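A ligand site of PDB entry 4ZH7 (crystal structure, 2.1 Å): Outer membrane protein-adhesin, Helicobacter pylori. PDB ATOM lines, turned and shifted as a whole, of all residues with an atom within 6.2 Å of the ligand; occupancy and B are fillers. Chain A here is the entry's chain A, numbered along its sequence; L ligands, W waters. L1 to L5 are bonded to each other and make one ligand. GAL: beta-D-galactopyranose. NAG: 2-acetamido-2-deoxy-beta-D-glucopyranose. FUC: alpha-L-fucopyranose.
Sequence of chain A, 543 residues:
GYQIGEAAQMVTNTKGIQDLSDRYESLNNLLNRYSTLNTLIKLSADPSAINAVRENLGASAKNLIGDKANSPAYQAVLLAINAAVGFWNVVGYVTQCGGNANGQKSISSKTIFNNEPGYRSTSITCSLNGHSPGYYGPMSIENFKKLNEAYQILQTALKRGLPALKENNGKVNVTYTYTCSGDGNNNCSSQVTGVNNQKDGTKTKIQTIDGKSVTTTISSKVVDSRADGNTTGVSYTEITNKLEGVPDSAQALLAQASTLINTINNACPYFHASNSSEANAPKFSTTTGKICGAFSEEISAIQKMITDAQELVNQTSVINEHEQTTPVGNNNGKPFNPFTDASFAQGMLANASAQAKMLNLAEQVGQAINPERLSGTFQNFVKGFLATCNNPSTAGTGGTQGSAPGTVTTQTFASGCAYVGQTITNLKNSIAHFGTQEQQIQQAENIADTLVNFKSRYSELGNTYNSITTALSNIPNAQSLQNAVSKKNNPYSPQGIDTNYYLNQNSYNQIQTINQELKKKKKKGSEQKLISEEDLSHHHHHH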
ATOM      1  N   SER A 108      -3.224 -28.139  13.939  1.00  0.00           N
ATOM      2  CA  SER A 108      -2.749 -28.489  12.594  1.00  0.00           C
ATOM      3  C   SER A 108      -3.002 -27.384  11.585  1.00  0.00           C
ATOM      4  O   SER A 108      -3.794 -27.527  10.637  1.00  0.00           O
ATOM      5  CB  SER A 108      -3.435 -29.801  12.130  1.00  0.00           C
ATOM      6  OG  SER A 108      -4.838 -29.724  12.372  1.00  0.00           O
ATOM      7  N   LYS A 110      -1.086 -25.024   8.932  1.00  0.00           N
ATOM      8  CA  LYS A 110       0.060 -24.777   8.054  1.00  0.00           C
ATOM      9  C   LYS A 110      -0.271 -23.510   7.220  1.00  0.00           C
ATOM     10  O   LYS A 110      -1.235 -23.486   6.461  1.00  0.00           O
ATOM     11  CB  LYS A 110       0.325 -25.978   7.170  1.00  0.00           C
ATOM     12  CG  LYS A 110       1.502 -25.808   6.239  1.00  0.00           C
ATOM     13  CD  LYS A 110       1.779 -27.002   5.324  1.00  0.00           C
ATOM     14  CE  LYS A 110       2.440 -28.165   6.095  1.00  0.00           C
ATOM     15  NZ  LYS A 110       3.056 -29.160   5.188  1.00  0.00           N
ATOM     16  N   CYS A 180      -3.336 -21.077   3.473  1.00  0.00           N
ATOM     17  CA  CYS A 180      -3.729 -21.804   4.714  1.00  0.00           C
ATOM     18  C   CYS A 180      -4.219 -23.227   4.321  1.00  0.00           C
ATOM     19  O   CYS A 180      -5.008 -23.414   3.363  1.00  0.00           O
ATOM     20  CB  CYS A 180      -4.899 -21.127   5.473  1.00  0.00           C
ATOM     21  SG  CYS A 180      -4.512 -19.478   6.103  1.00  0.00           S
ATOM     22  N   SER A 181      -3.712 -24.231   5.050  1.00  0.00           N
ATOM     23  CA  SER A 181      -4.114 -25.622   4.894  1.00  0.00           C
ATOM     24  C   SER A 181      -4.061 -26.247   6.267  1.00  0.00           C
ATOM     25  O   SER A 181      -3.611 -25.612   7.234  1.00  0.00           O
ATOM     26  CB  SER A 181      -3.262 -26.390   3.868  1.00  0.00           C
ATOM     27  OG  SER A 181      -1.916 -26.408   4.230  1.00  0.00           O
ATOM     28  N   GLY A 182      -4.630 -27.440   6.370  1.00  0.00           N
ATOM     29  CA  GLY A 182      -4.769 -28.151   7.610  1.00  0.00           C
ATOM     30  C   GLY A 182      -6.098 -27.917   8.291  1.00  0.00           C
ATOM     31  O   GLY A 182      -6.670 -26.806   8.246  1.00  0.00           O
ATOM     32  N   ASP A 183      -6.583 -28.989   8.932  1.00  0.00           N
ATOM     33  CA  ASP A 183      -7.854 -28.939   9.668  1.00  0.00           C
ATOM     34  C   ASP A 183      -7.802 -27.918  10.797  1.00  0.00           C
ATOM     35  O   ASP A 183      -6.866 -27.909  11.577  1.00  0.00           O
ATOM     36  CB  ASP A 183      -8.191 -30.340  10.250  1.00  0.00           C
ATOM     37  CG  ASP A 183      -9.582 -30.383  10.850  1.00  0.00           C
ATOM     38  OD1 ASP A 183     -10.521 -29.906  10.205  1.00  0.00           O
ATOM     39  OD2 ASP A 183      -9.757 -30.876  11.974  1.00  0.00           O
ATOM     40  N   GLY A 184      -8.794 -27.037  10.849  1.00  0.00           N
ATOM     41  CA  GLY A 184      -8.883 -25.971  11.834  1.00  0.00           C
ATOM     42  C   GLY A 184      -8.061 -24.697  11.601  1.00  0.00           C
ATOM     43  O   GLY A 184      -7.970 -23.875  12.506  1.00  0.00           O
ATOM     44  N   ASN A 185      -7.400 -24.549  10.443  1.00  0.00           N
ATOM     45  CA  ASN A 185      -6.616 -23.313  10.180  1.00  0.00           C
ATOM     46  C   ASN A 185      -7.585 -22.187   9.813  1.00  0.00           C
ATOM     47  O   ASN A 185      -8.316 -22.301   8.783  1.00  0.00           O
ATOM     48  CB  ASN A 185      -5.626 -23.534   9.054  1.00  0.00           C
ATOM     49  CG  ASN A 185      -4.583 -22.422   8.960  1.00  0.00           C
ATOM     50  OD1 ASN A 185      -4.778 -21.350   9.449  1.00  0.00           O
ATOM     51  ND2 ASN A 185      -3.463 -22.702   8.348  1.00  0.00           N
ATOM     52  N   ASN A 186      -7.624 -21.142  10.656  1.00  0.00           N
ATOM     53  CA  ASN A 186      -8.542 -20.023  10.507  1.00  0.00           C
ATOM     54  C   ASN A 186      -7.847 -18.699  10.139  1.00  0.00           C
ATOM     55  O   ASN A 186      -8.460 -17.624  10.207  1.00  0.00           O
ATOM     56  CB  ASN A 186      -9.365 -19.803  11.756  1.00  0.00           C
ATOM     57  CG  ASN A 186      -8.528 -19.440  12.934  1.00  0.00           C
ATOM     58  OD1 ASN A 186      -7.278 -19.293  12.821  1.00  0.00           O
ATOM     59  ND2 ASN A 186      -9.155 -19.256  14.065  1.00  0.00           N
ATOM     60  N   CYS A 188      -7.010 -17.773   7.259  1.00  0.00           N
ATOM     61  CA  CYS A 188      -7.496 -17.298   5.964  1.00  0.00           C
ATOM     62  C   CYS A 188      -9.039 -17.242   5.911  1.00  0.00           C
ATOM     63  O   CYS A 188      -9.605 -17.208   4.825  1.00  0.00           O
ATOM     64  CB  CYS A 188      -6.966 -18.122   4.761  1.00  0.00           C
ATOM     65  SG  CYS A 188      -5.182 -18.275   4.572  1.00  0.00           S
ATOM     66  N   ASN A 197     -16.743 -13.968   0.903  1.00  0.00           N
ATOM     67  CA  ASN A 197     -16.839 -15.428   0.713  1.00  0.00           C
ATOM     68  C   ASN A 197     -15.432 -16.044   0.576  1.00  0.00           C
ATOM     69  O   ASN A 197     -14.739 -15.789  -0.373  1.00  0.00           O
ATOM     70  CB  ASN A 197     -17.644 -15.698  -0.566  1.00  0.00           C
ATOM     71  CG  ASN A 197     -17.752 -17.197  -0.916  1.00  0.00           C
ATOM     72  OD1 ASN A 197     -17.502 -18.098  -0.095  1.00  0.00           O
ATOM     73  ND2 ASN A 197     -18.159 -17.474  -2.153  1.00  0.00           N
ATOM     74  N   GLN A 198     -15.029 -16.876   1.531  1.00  0.00           N
ATOM     75  CA  GLN A 198     -13.708 -17.501   1.477  1.00  0.00           C
ATOM     76  C   GLN A 198     -13.374 -18.268   0.204  1.00  0.00           C
ATOM     77  O   GLN A 198     -12.223 -18.247  -0.256  1.00  0.00           O
ATOM     78  CB  GLN A 198     -13.559 -18.456   2.663  1.00  0.00           C
ATOM     79  CG  GLN A 198     -12.125 -18.919   2.926  1.00  0.00           C
ATOM     80  CD  GLN A 198     -12.022 -19.855   4.133  1.00  0.00           C
ATOM     81  OE1 GLN A 198     -12.749 -19.741   5.107  1.00  0.00           O
ATOM     82  NE2 GLN A 198     -11.077 -20.750   4.073  1.00  0.00           N
ATOM     83  N   LYS A 199     -14.326 -19.023  -0.343  1.00  0.00           N
ATOM     84  CA  LYS A 199     -14.076 -19.875  -1.523  1.00  0.00           C
ATOM     85  C   LYS A 199     -13.766 -19.060  -2.750  1.00  0.00           C
ATOM     86  O   LYS A 199     -13.116 -19.531  -3.724  1.00  0.00           O
ATOM     87  CB  LYS A 199     -15.317 -20.664  -1.947  1.00  0.00           C
ATOM     88  CG  LYS A 199     -16.036 -21.532  -0.934  1.00  0.00           C
ATOM     89  CD  LYS A 199     -17.150 -22.352  -1.594  1.00  0.00           C
ATOM     90  CE  LYS A 199     -16.729 -22.918  -2.959  1.00  0.00           C
ATOM     91  NZ  LYS A 199     -17.742 -23.811  -3.615  1.00  0.00           N
ATOM     92  N   VAL A 222     -10.454 -20.855  -2.571  1.00  0.00           N
ATOM     93  CA  VAL A 222     -10.120 -22.201  -2.139  1.00  0.00           C
ATOM     94  C   VAL A 222      -9.763 -23.053  -3.354  1.00  0.00           C
ATOM     95  O   VAL A 222     -10.522 -23.090  -4.282  1.00  0.00           O
ATOM     96  CB  VAL A 222     -11.327 -22.801  -1.411  1.00  0.00           C
ATOM     97  CG1 VAL A 222     -11.214 -24.320  -1.231  1.00  0.00           C
ATOM     98  CG2 VAL A 222     -11.450 -22.107  -0.068  1.00  0.00           C
ATOM     99  N   VAL A 223      -8.607 -23.697  -3.330  1.00  0.00           N
ATOM    100  CA  VAL A 223      -8.192 -24.699  -4.319  1.00  0.00           C
ATOM    101  C   VAL A 223      -8.381 -26.061  -3.644  1.00  0.00           C
ATOM    102  O   VAL A 223      -7.777 -26.348  -2.582  1.00  0.00           O
ATOM    103  CB  VAL A 223      -6.709 -24.529  -4.702  1.00  0.00           C
ATOM    104  CG1 VAL A 223      -6.297 -25.499  -5.801  1.00  0.00           C
ATOM    105  CG2 VAL A 223      -6.395 -23.097  -5.162  1.00  0.00           C
ATOM    106  N   ASP A 224      -9.236 -26.888  -4.255  1.00  0.00           N
ATOM    107  CA  ASP A 224      -9.617 -28.174  -3.731  1.00  0.00           C
ATOM    108  C   ASP A 224      -8.472 -29.107  -4.000  1.00  0.00           C
ATOM    109  O   ASP A 224      -7.773 -28.909  -5.010  1.00  0.00           O
ATOM    110  CB  ASP A 224     -10.906 -28.731  -4.401  1.00  0.00           C
ATOM    111  CG  ASP A 224     -11.284 -30.094  -3.837  1.00  0.00           C
ATOM    112  OD1 ASP A 224     -11.673 -30.156  -2.650  1.00  0.00           O
ATOM    113  OD2 ASP A 224     -11.075 -31.109  -4.527  1.00  0.00           O
ATOM    114  N   SER A 225      -8.275 -30.095  -3.118  1.00  0.00           N
ATOM    115  CA  SER A 225      -7.188 -31.111  -3.235  1.00  0.00           C
ATOM    116  C   SER A 225      -7.165 -31.808  -4.594  1.00  0.00           C
ATOM    117  O   SER A 225      -6.088 -32.188  -5.065  1.00  0.00           O
ATOM    118  CB  SER A 225      -7.283 -32.206  -2.140  1.00  0.00           C
ATOM    119  OG  SER A 225      -8.504 -32.958  -2.245  1.00  0.00           O
ATOM    120  N   GLY A 233      -1.793 -32.303  -2.851  1.00  0.00           N
ATOM    121  CA  GLY A 233      -2.585 -33.338  -2.196  1.00  0.00           C
ATOM    122  C   GLY A 233      -3.455 -32.843  -1.062  1.00  0.00           C
ATOM    123  O   GLY A 233      -3.988 -33.647  -0.306  1.00  0.00           O
ATOM    124  N   VAL A 234      -3.620 -31.516  -0.942  1.00  0.00           N
ATOM    125  CA  VAL A 234      -4.569 -30.990   0.056  1.00  0.00           C
ATOM    126  C   VAL A 234      -5.297 -29.778  -0.501  1.00  0.00           C
ATOM    127  O   VAL A 234      -4.795 -29.091  -1.387  1.00  0.00           O
ATOM    128  CB  VAL A 234      -3.917 -30.626   1.432  1.00  0.00           C
ATOM    129  CG1 VAL A 234      -3.350 -31.881   2.136  1.00  0.00           C
ATOM    130  CG2 VAL A 234      -2.798 -29.588   1.284  1.00  0.00           C
ATOM    131  N   SER A 235      -6.475 -29.551   0.023  1.00  0.00           N
ATOM    132  CA  SER A 235      -7.185 -28.311  -0.164  1.00  0.00           C
ATOM    133  C   SER A 235      -6.508 -27.165   0.588  1.00  0.00           C
ATOM    134  O   SER A 235      -6.041 -27.343   1.707  1.00  0.00           O
ATOM    135  CB  SER A 235      -8.585 -28.448   0.336  1.00  0.00           C
ATOM    136  OG  SER A 235      -9.282 -29.371  -0.454  1.00  0.00           O
ATOM    137  N   TYR A 236      -6.454 -25.985  -0.023  1.00  0.00           N
ATOM    138  CA  TYR A 236      -5.907 -24.831   0.645  1.00  0.00           C
ATOM    139  C   TYR A 236      -6.654 -23.578   0.260  1.00  0.00           C
ATOM    140  O   TYR A 236      -7.285 -23.549  -0.794  1.00  0.00           O
ATOM    141  CB  TYR A 236      -4.405 -24.733   0.351  1.00  0.00           C
ATOM    142  CG  TYR A 236      -3.974 -24.506  -1.097  1.00  0.00           C
ATOM    143  CD1 TYR A 236      -3.815 -23.217  -1.572  1.00  0.00           C
ATOM    144  CD2 TYR A 236      -3.661 -25.564  -1.962  1.00  0.00           C
ATOM    145  CE1 TYR A 236      -3.411 -22.968  -2.868  1.00  0.00           C
ATOM    146  CE2 TYR A 236      -3.284 -25.326  -3.288  1.00  0.00           C
ATOM    147  CZ  TYR A 236      -3.144 -24.007  -3.711  1.00  0.00           C
ATOM    148  OH  TYR A 236      -2.760 -23.652  -4.975  1.00  0.00           O
ATOM    149  N   THR A 237      -6.587 -22.542   1.118  1.00  0.00           N
ATOM    150  CA  THR A 237      -7.081 -21.228   0.772  1.00  0.00           C
ATOM    151  C   THR A 237      -5.901 -20.334   0.409  1.00  0.00           C
ATOM    152  O   THR A 237      -4.896 -20.332   1.126  1.00  0.00           O
ATOM    153  CB  THR A 237      -7.812 -20.605   1.941  1.00  0.00           C
ATOM    154  OG1 THR A 237      -8.822 -21.522   2.446  1.00  0.00           O
ATOM    155  CG2 THR A 237      -8.429 -19.263   1.490  1.00  0.00           C
HETATM  156  C1  GAL L   1      -8.099 -33.633   2.436  1.00  0.00           C
HETATM  157  C2  GAL L   1      -8.663 -32.335   1.882  1.00  0.00           C
HETATM  158  C3  GAL L   1      -9.587 -31.518   2.801  1.00  0.00           C
HETATM  159  C4  GAL L   1     -10.070 -32.210   4.127  1.00  0.00           C
HETATM  160  C5  GAL L   1      -9.432 -33.592   4.446  1.00  0.00           C
HETATM  161  C6  GAL L   1     -10.325 -34.500   5.317  1.00  0.00           C
HETATM  162  O1  GAL L   1      -7.558 -34.417   1.353  1.00  0.00           O
HETATM  163  O2  GAL L   1      -7.529 -31.528   1.961  1.00  0.00           O
HETATM  164  O3  GAL L   1     -10.466 -30.884   1.885  1.00  0.00           O
HETATM  165  O4  GAL L   1     -11.465 -32.158   4.268  1.00  0.00           O
HETATM  166  O5  GAL L   1      -9.102 -34.239   3.224  1.00  0.00           O
HETATM  167  O6  GAL L   1      -9.524 -35.222   6.236  1.00  0.00           O
HETATM  168  C1  NAG L   2     -11.556 -29.951   2.162  1.00  0.00           C
HETATM  169  C2  NAG L   2     -11.406 -28.744   3.118  1.00  0.00           C
HETATM  170  C3  NAG L   2     -12.675 -27.925   3.101  1.00  0.00           C
HETATM  171  C4  NAG L   2     -13.130 -27.625   1.663  1.00  0.00           C
HETATM  172  C5  NAG L   2     -13.244 -28.921   0.854  1.00  0.00           C
HETATM  173  C6  NAG L   2     -13.735 -28.660  -0.564  1.00  0.00           C
HETATM  174  C7  NAG L   2      -9.844 -28.858   4.981  1.00  0.00           C
HETATM  175  C8  NAG L   2      -9.604 -29.213   6.428  1.00  0.00           C
HETATM  176  N2  NAG L   2     -11.089 -29.033   4.513  1.00  0.00           N
HETATM  177  O3  NAG L   2     -12.508 -26.727   3.806  1.00  0.00           O
HETATM  178  O4  NAG L   2     -14.431 -27.116   1.774  1.00  0.00           O
HETATM  179  O5  NAG L   2     -11.943 -29.494   0.852  1.00  0.00           O
HETATM  180  O6  NAG L   2     -12.625 -28.323  -1.359  1.00  0.00           O
HETATM  181  O7  NAG L   2      -8.914 -28.417   4.264  1.00  0.00           O
HETATM  182  C1  GAL L   3     -13.222 -26.691   5.039  1.00  0.00           C
HETATM  183  C2  GAL L   3     -12.761 -25.438   5.792  1.00  0.00           C
HETATM  184  C3  GAL L   3     -13.542 -25.278   7.079  1.00  0.00           C
HETATM  185  C4  GAL L   3     -15.072 -25.358   6.844  1.00  0.00           C
HETATM  186  C5  GAL L   3     -15.371 -26.643   6.134  1.00  0.00           C
HETATM  187  C6  GAL L   3     -16.860 -26.859   5.886  1.00  0.00           C
HETATM  188  O2  GAL L   3     -11.360 -25.467   6.041  1.00  0.00           O
HETATM  189  O3  GAL L   3     -13.237 -24.007   7.559  1.00  0.00           O
HETATM  190  O4  GAL L   3     -15.509 -24.350   5.972  1.00  0.00           O
HETATM  191  O5  GAL L   3     -14.652 -26.692   4.901  1.00  0.00           O
HETATM  192  O6  GAL L   3     -16.874 -28.149   5.314  1.00  0.00           O
HETATM  193  C1  FUC L   4     -14.760 -25.892   1.110  1.00  0.00           C
HETATM  194  C2  FUC L   4     -16.257 -25.814   0.695  1.00  0.00           C
HETATM  195  C3  FUC L   4     -16.923 -25.452   2.029  1.00  0.00           C
HETATM  196  C4  FUC L   4     -16.298 -24.104   2.476  1.00  0.00           C
HETATM  197  C5  FUC L   4     -14.732 -24.105   2.558  1.00  0.00           C
HETATM  198  C6  FUC L   4     -14.130 -22.759   3.005  1.00  0.00           C
HETATM  199  O2  FUC L   4     -16.731 -27.060   0.283  1.00  0.00           O
HETATM  200  O3  FUC L   4     -18.324 -25.367   1.981  1.00  0.00           O
HETATM  201  O4  FUC L   4     -16.735 -23.194   1.523  1.00  0.00           O
HETATM  202  O5  FUC L   4     -14.162 -24.610   1.337  1.00  0.00           O
HETATM  203  C1  FUC L   5     -10.721 -24.207   5.716  1.00  0.00           C
HETATM  204  C2  FUC L   5      -9.342 -24.095   6.347  1.00  0.00           C
HETATM  205  C3  FUC L   5      -8.364 -25.083   5.735  1.00  0.00           C
HETATM  206  C4  FUC L   5      -8.323 -24.906   4.203  1.00  0.00           C
HETATM  207  C5  FUC L   5      -9.767 -24.979   3.695  1.00  0.00           C
HETATM  208  C6  FUC L   5      -9.844 -24.777   2.178  1.00  0.00           C
HETATM  209  O2  FUC L   5      -9.385 -24.262   7.749  1.00  0.00           O
HETATM  210  O3  FUC L   5      -7.069 -24.928   6.290  1.00  0.00           O
HETATM  211  O4  FUC L   5      -7.707 -23.669   3.828  1.00  0.00           O
HETATM  212  O5  FUC L   5     -10.591 -24.043   4.330  1.00  0.00           O
HETATM  213  O   HOH W   1     -16.737 -20.056   2.074  1.00  0.00           O
HETATM  214  O   HOH W   2     -19.203 -26.799  -1.749  1.00  0.00           O
HETATM  215  O   HOH W   3     -10.591 -32.149  -1.225  1.00  0.00           O
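Water W1 lies within hydrogen-bond range of OD1 of Asn 197 (3.0 Å) and O4 of FUC L4 (3.2 Å).
Water W3 lies within hydrogen-bond range of the side-chain hydroxyl (OG) of Ser 225 (2.5 Å), the side-chain carboxylate (OD1) of Asp 224 (2.7 Å), the side-chain hydroxyl (OG) of Ser 235 (3.2 Å) and an oxygen (O3) of GAL L1 (3.4 Å).
Merely in contact with the ligand: Lys 199 (3.0 Å), Ser 181 (3.3 Å), Val 234 (3.6 Å), Asp 183 (3.7 Å), Val 222 (3.7 Å), Tyr 236 (3.7 Å) and Ser 225 (3.996 Å).
14 residues have an atom within 4 Å of the ligand: Cys 180, Ser 181, Gly 182, Asp 183, Asn 185, Gln 198, Lys 199, Val 222, Asp 224, Ser 225, Val 234, Ser 235, Tyr 236 and Thr 237.
The nearest printed residue that does not touch the ligand is Gly 233 (4.01 Å).
The side-chain amide nitrogen (ND2) of Asn 185 is in hydrogen-bond range of the backbone carbonyl oxygen (O) of Lys 110, 3.0 Å away.
O of Cys 180 is in hydrogen-bond range of N of Thr 237.
The side-chain sulfur (SG) of Cys 180 forms a disulfide with the side-chain sulfur (SG) of Cys 188 (2.1 Å).
The backbone NH (N) of Ser 225 sits at hydrogen-bond distance from the side-chain hydroxyl (OG) of Ser 235 (2.9 Å).
O of Lys 199 is in hydrogen-bond range of N of Val 222 (3.2 Å).
The side-chain amide oxygen (OD1) of Asn 197 sits close to the backbone NH (N) of Lys 199 (3.3 Å).
The backbone NH of Ser 181 is in hydrogen-bond range of the backbone carbonyl oxygen of Lys 110 (2.9 Å).
The backbone NH (N) of Val 223 sits at hydrogen-bond distance from the backbone carbonyl oxygen (O) of Tyr 236 (2.9 Å).
OD1 of Asp 224 is in hydrogen-bond range of O6 of NAG L2, 2.4 Å away.
N of Asn 185 lies within hydrogen-bond range of O2 of FUC L5 (3.4 Å).
An oxygen (O2) of FUC L5 lies within hydrogen-bond range of the backbone carbonyl oxygen (O) of Asn 185 (2.5 Å).
O of Gly 182 sits at hydrogen-bond distance from O3 of FUC L5, 2.7 Å away.
The backbone carbonyl oxygen (O) of Cys 180 sits at hydrogen-bond distance from an oxygen (O4) of FUC L5 (2.8 Å).
The backbone NH (N) of Thr 237 sits at hydrogen-bond distance from an oxygen (O4) of FUC L5 (3.1 Å).
An oxygen (O4) of FUC L5 is in hydrogen-bond range of the side-chain hydroxyl (OG1) of Thr 237, at 2.8 Å.
The backbone NH of Ser 235 lies within hydrogen-bond range of an oxygen (O2) of GAL L1, 3.0 Å away.
The side-chain hydroxyl of Ser 235 is in hydrogen-bond range of an oxygen (O5) of NAG L2, 3.0 Å away.
An oxygen (O5) of FUC L5 sits at hydrogen-bond distance from the side-chain amide nitrogen (NE2) of Gln 198, 3.3 Å away.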
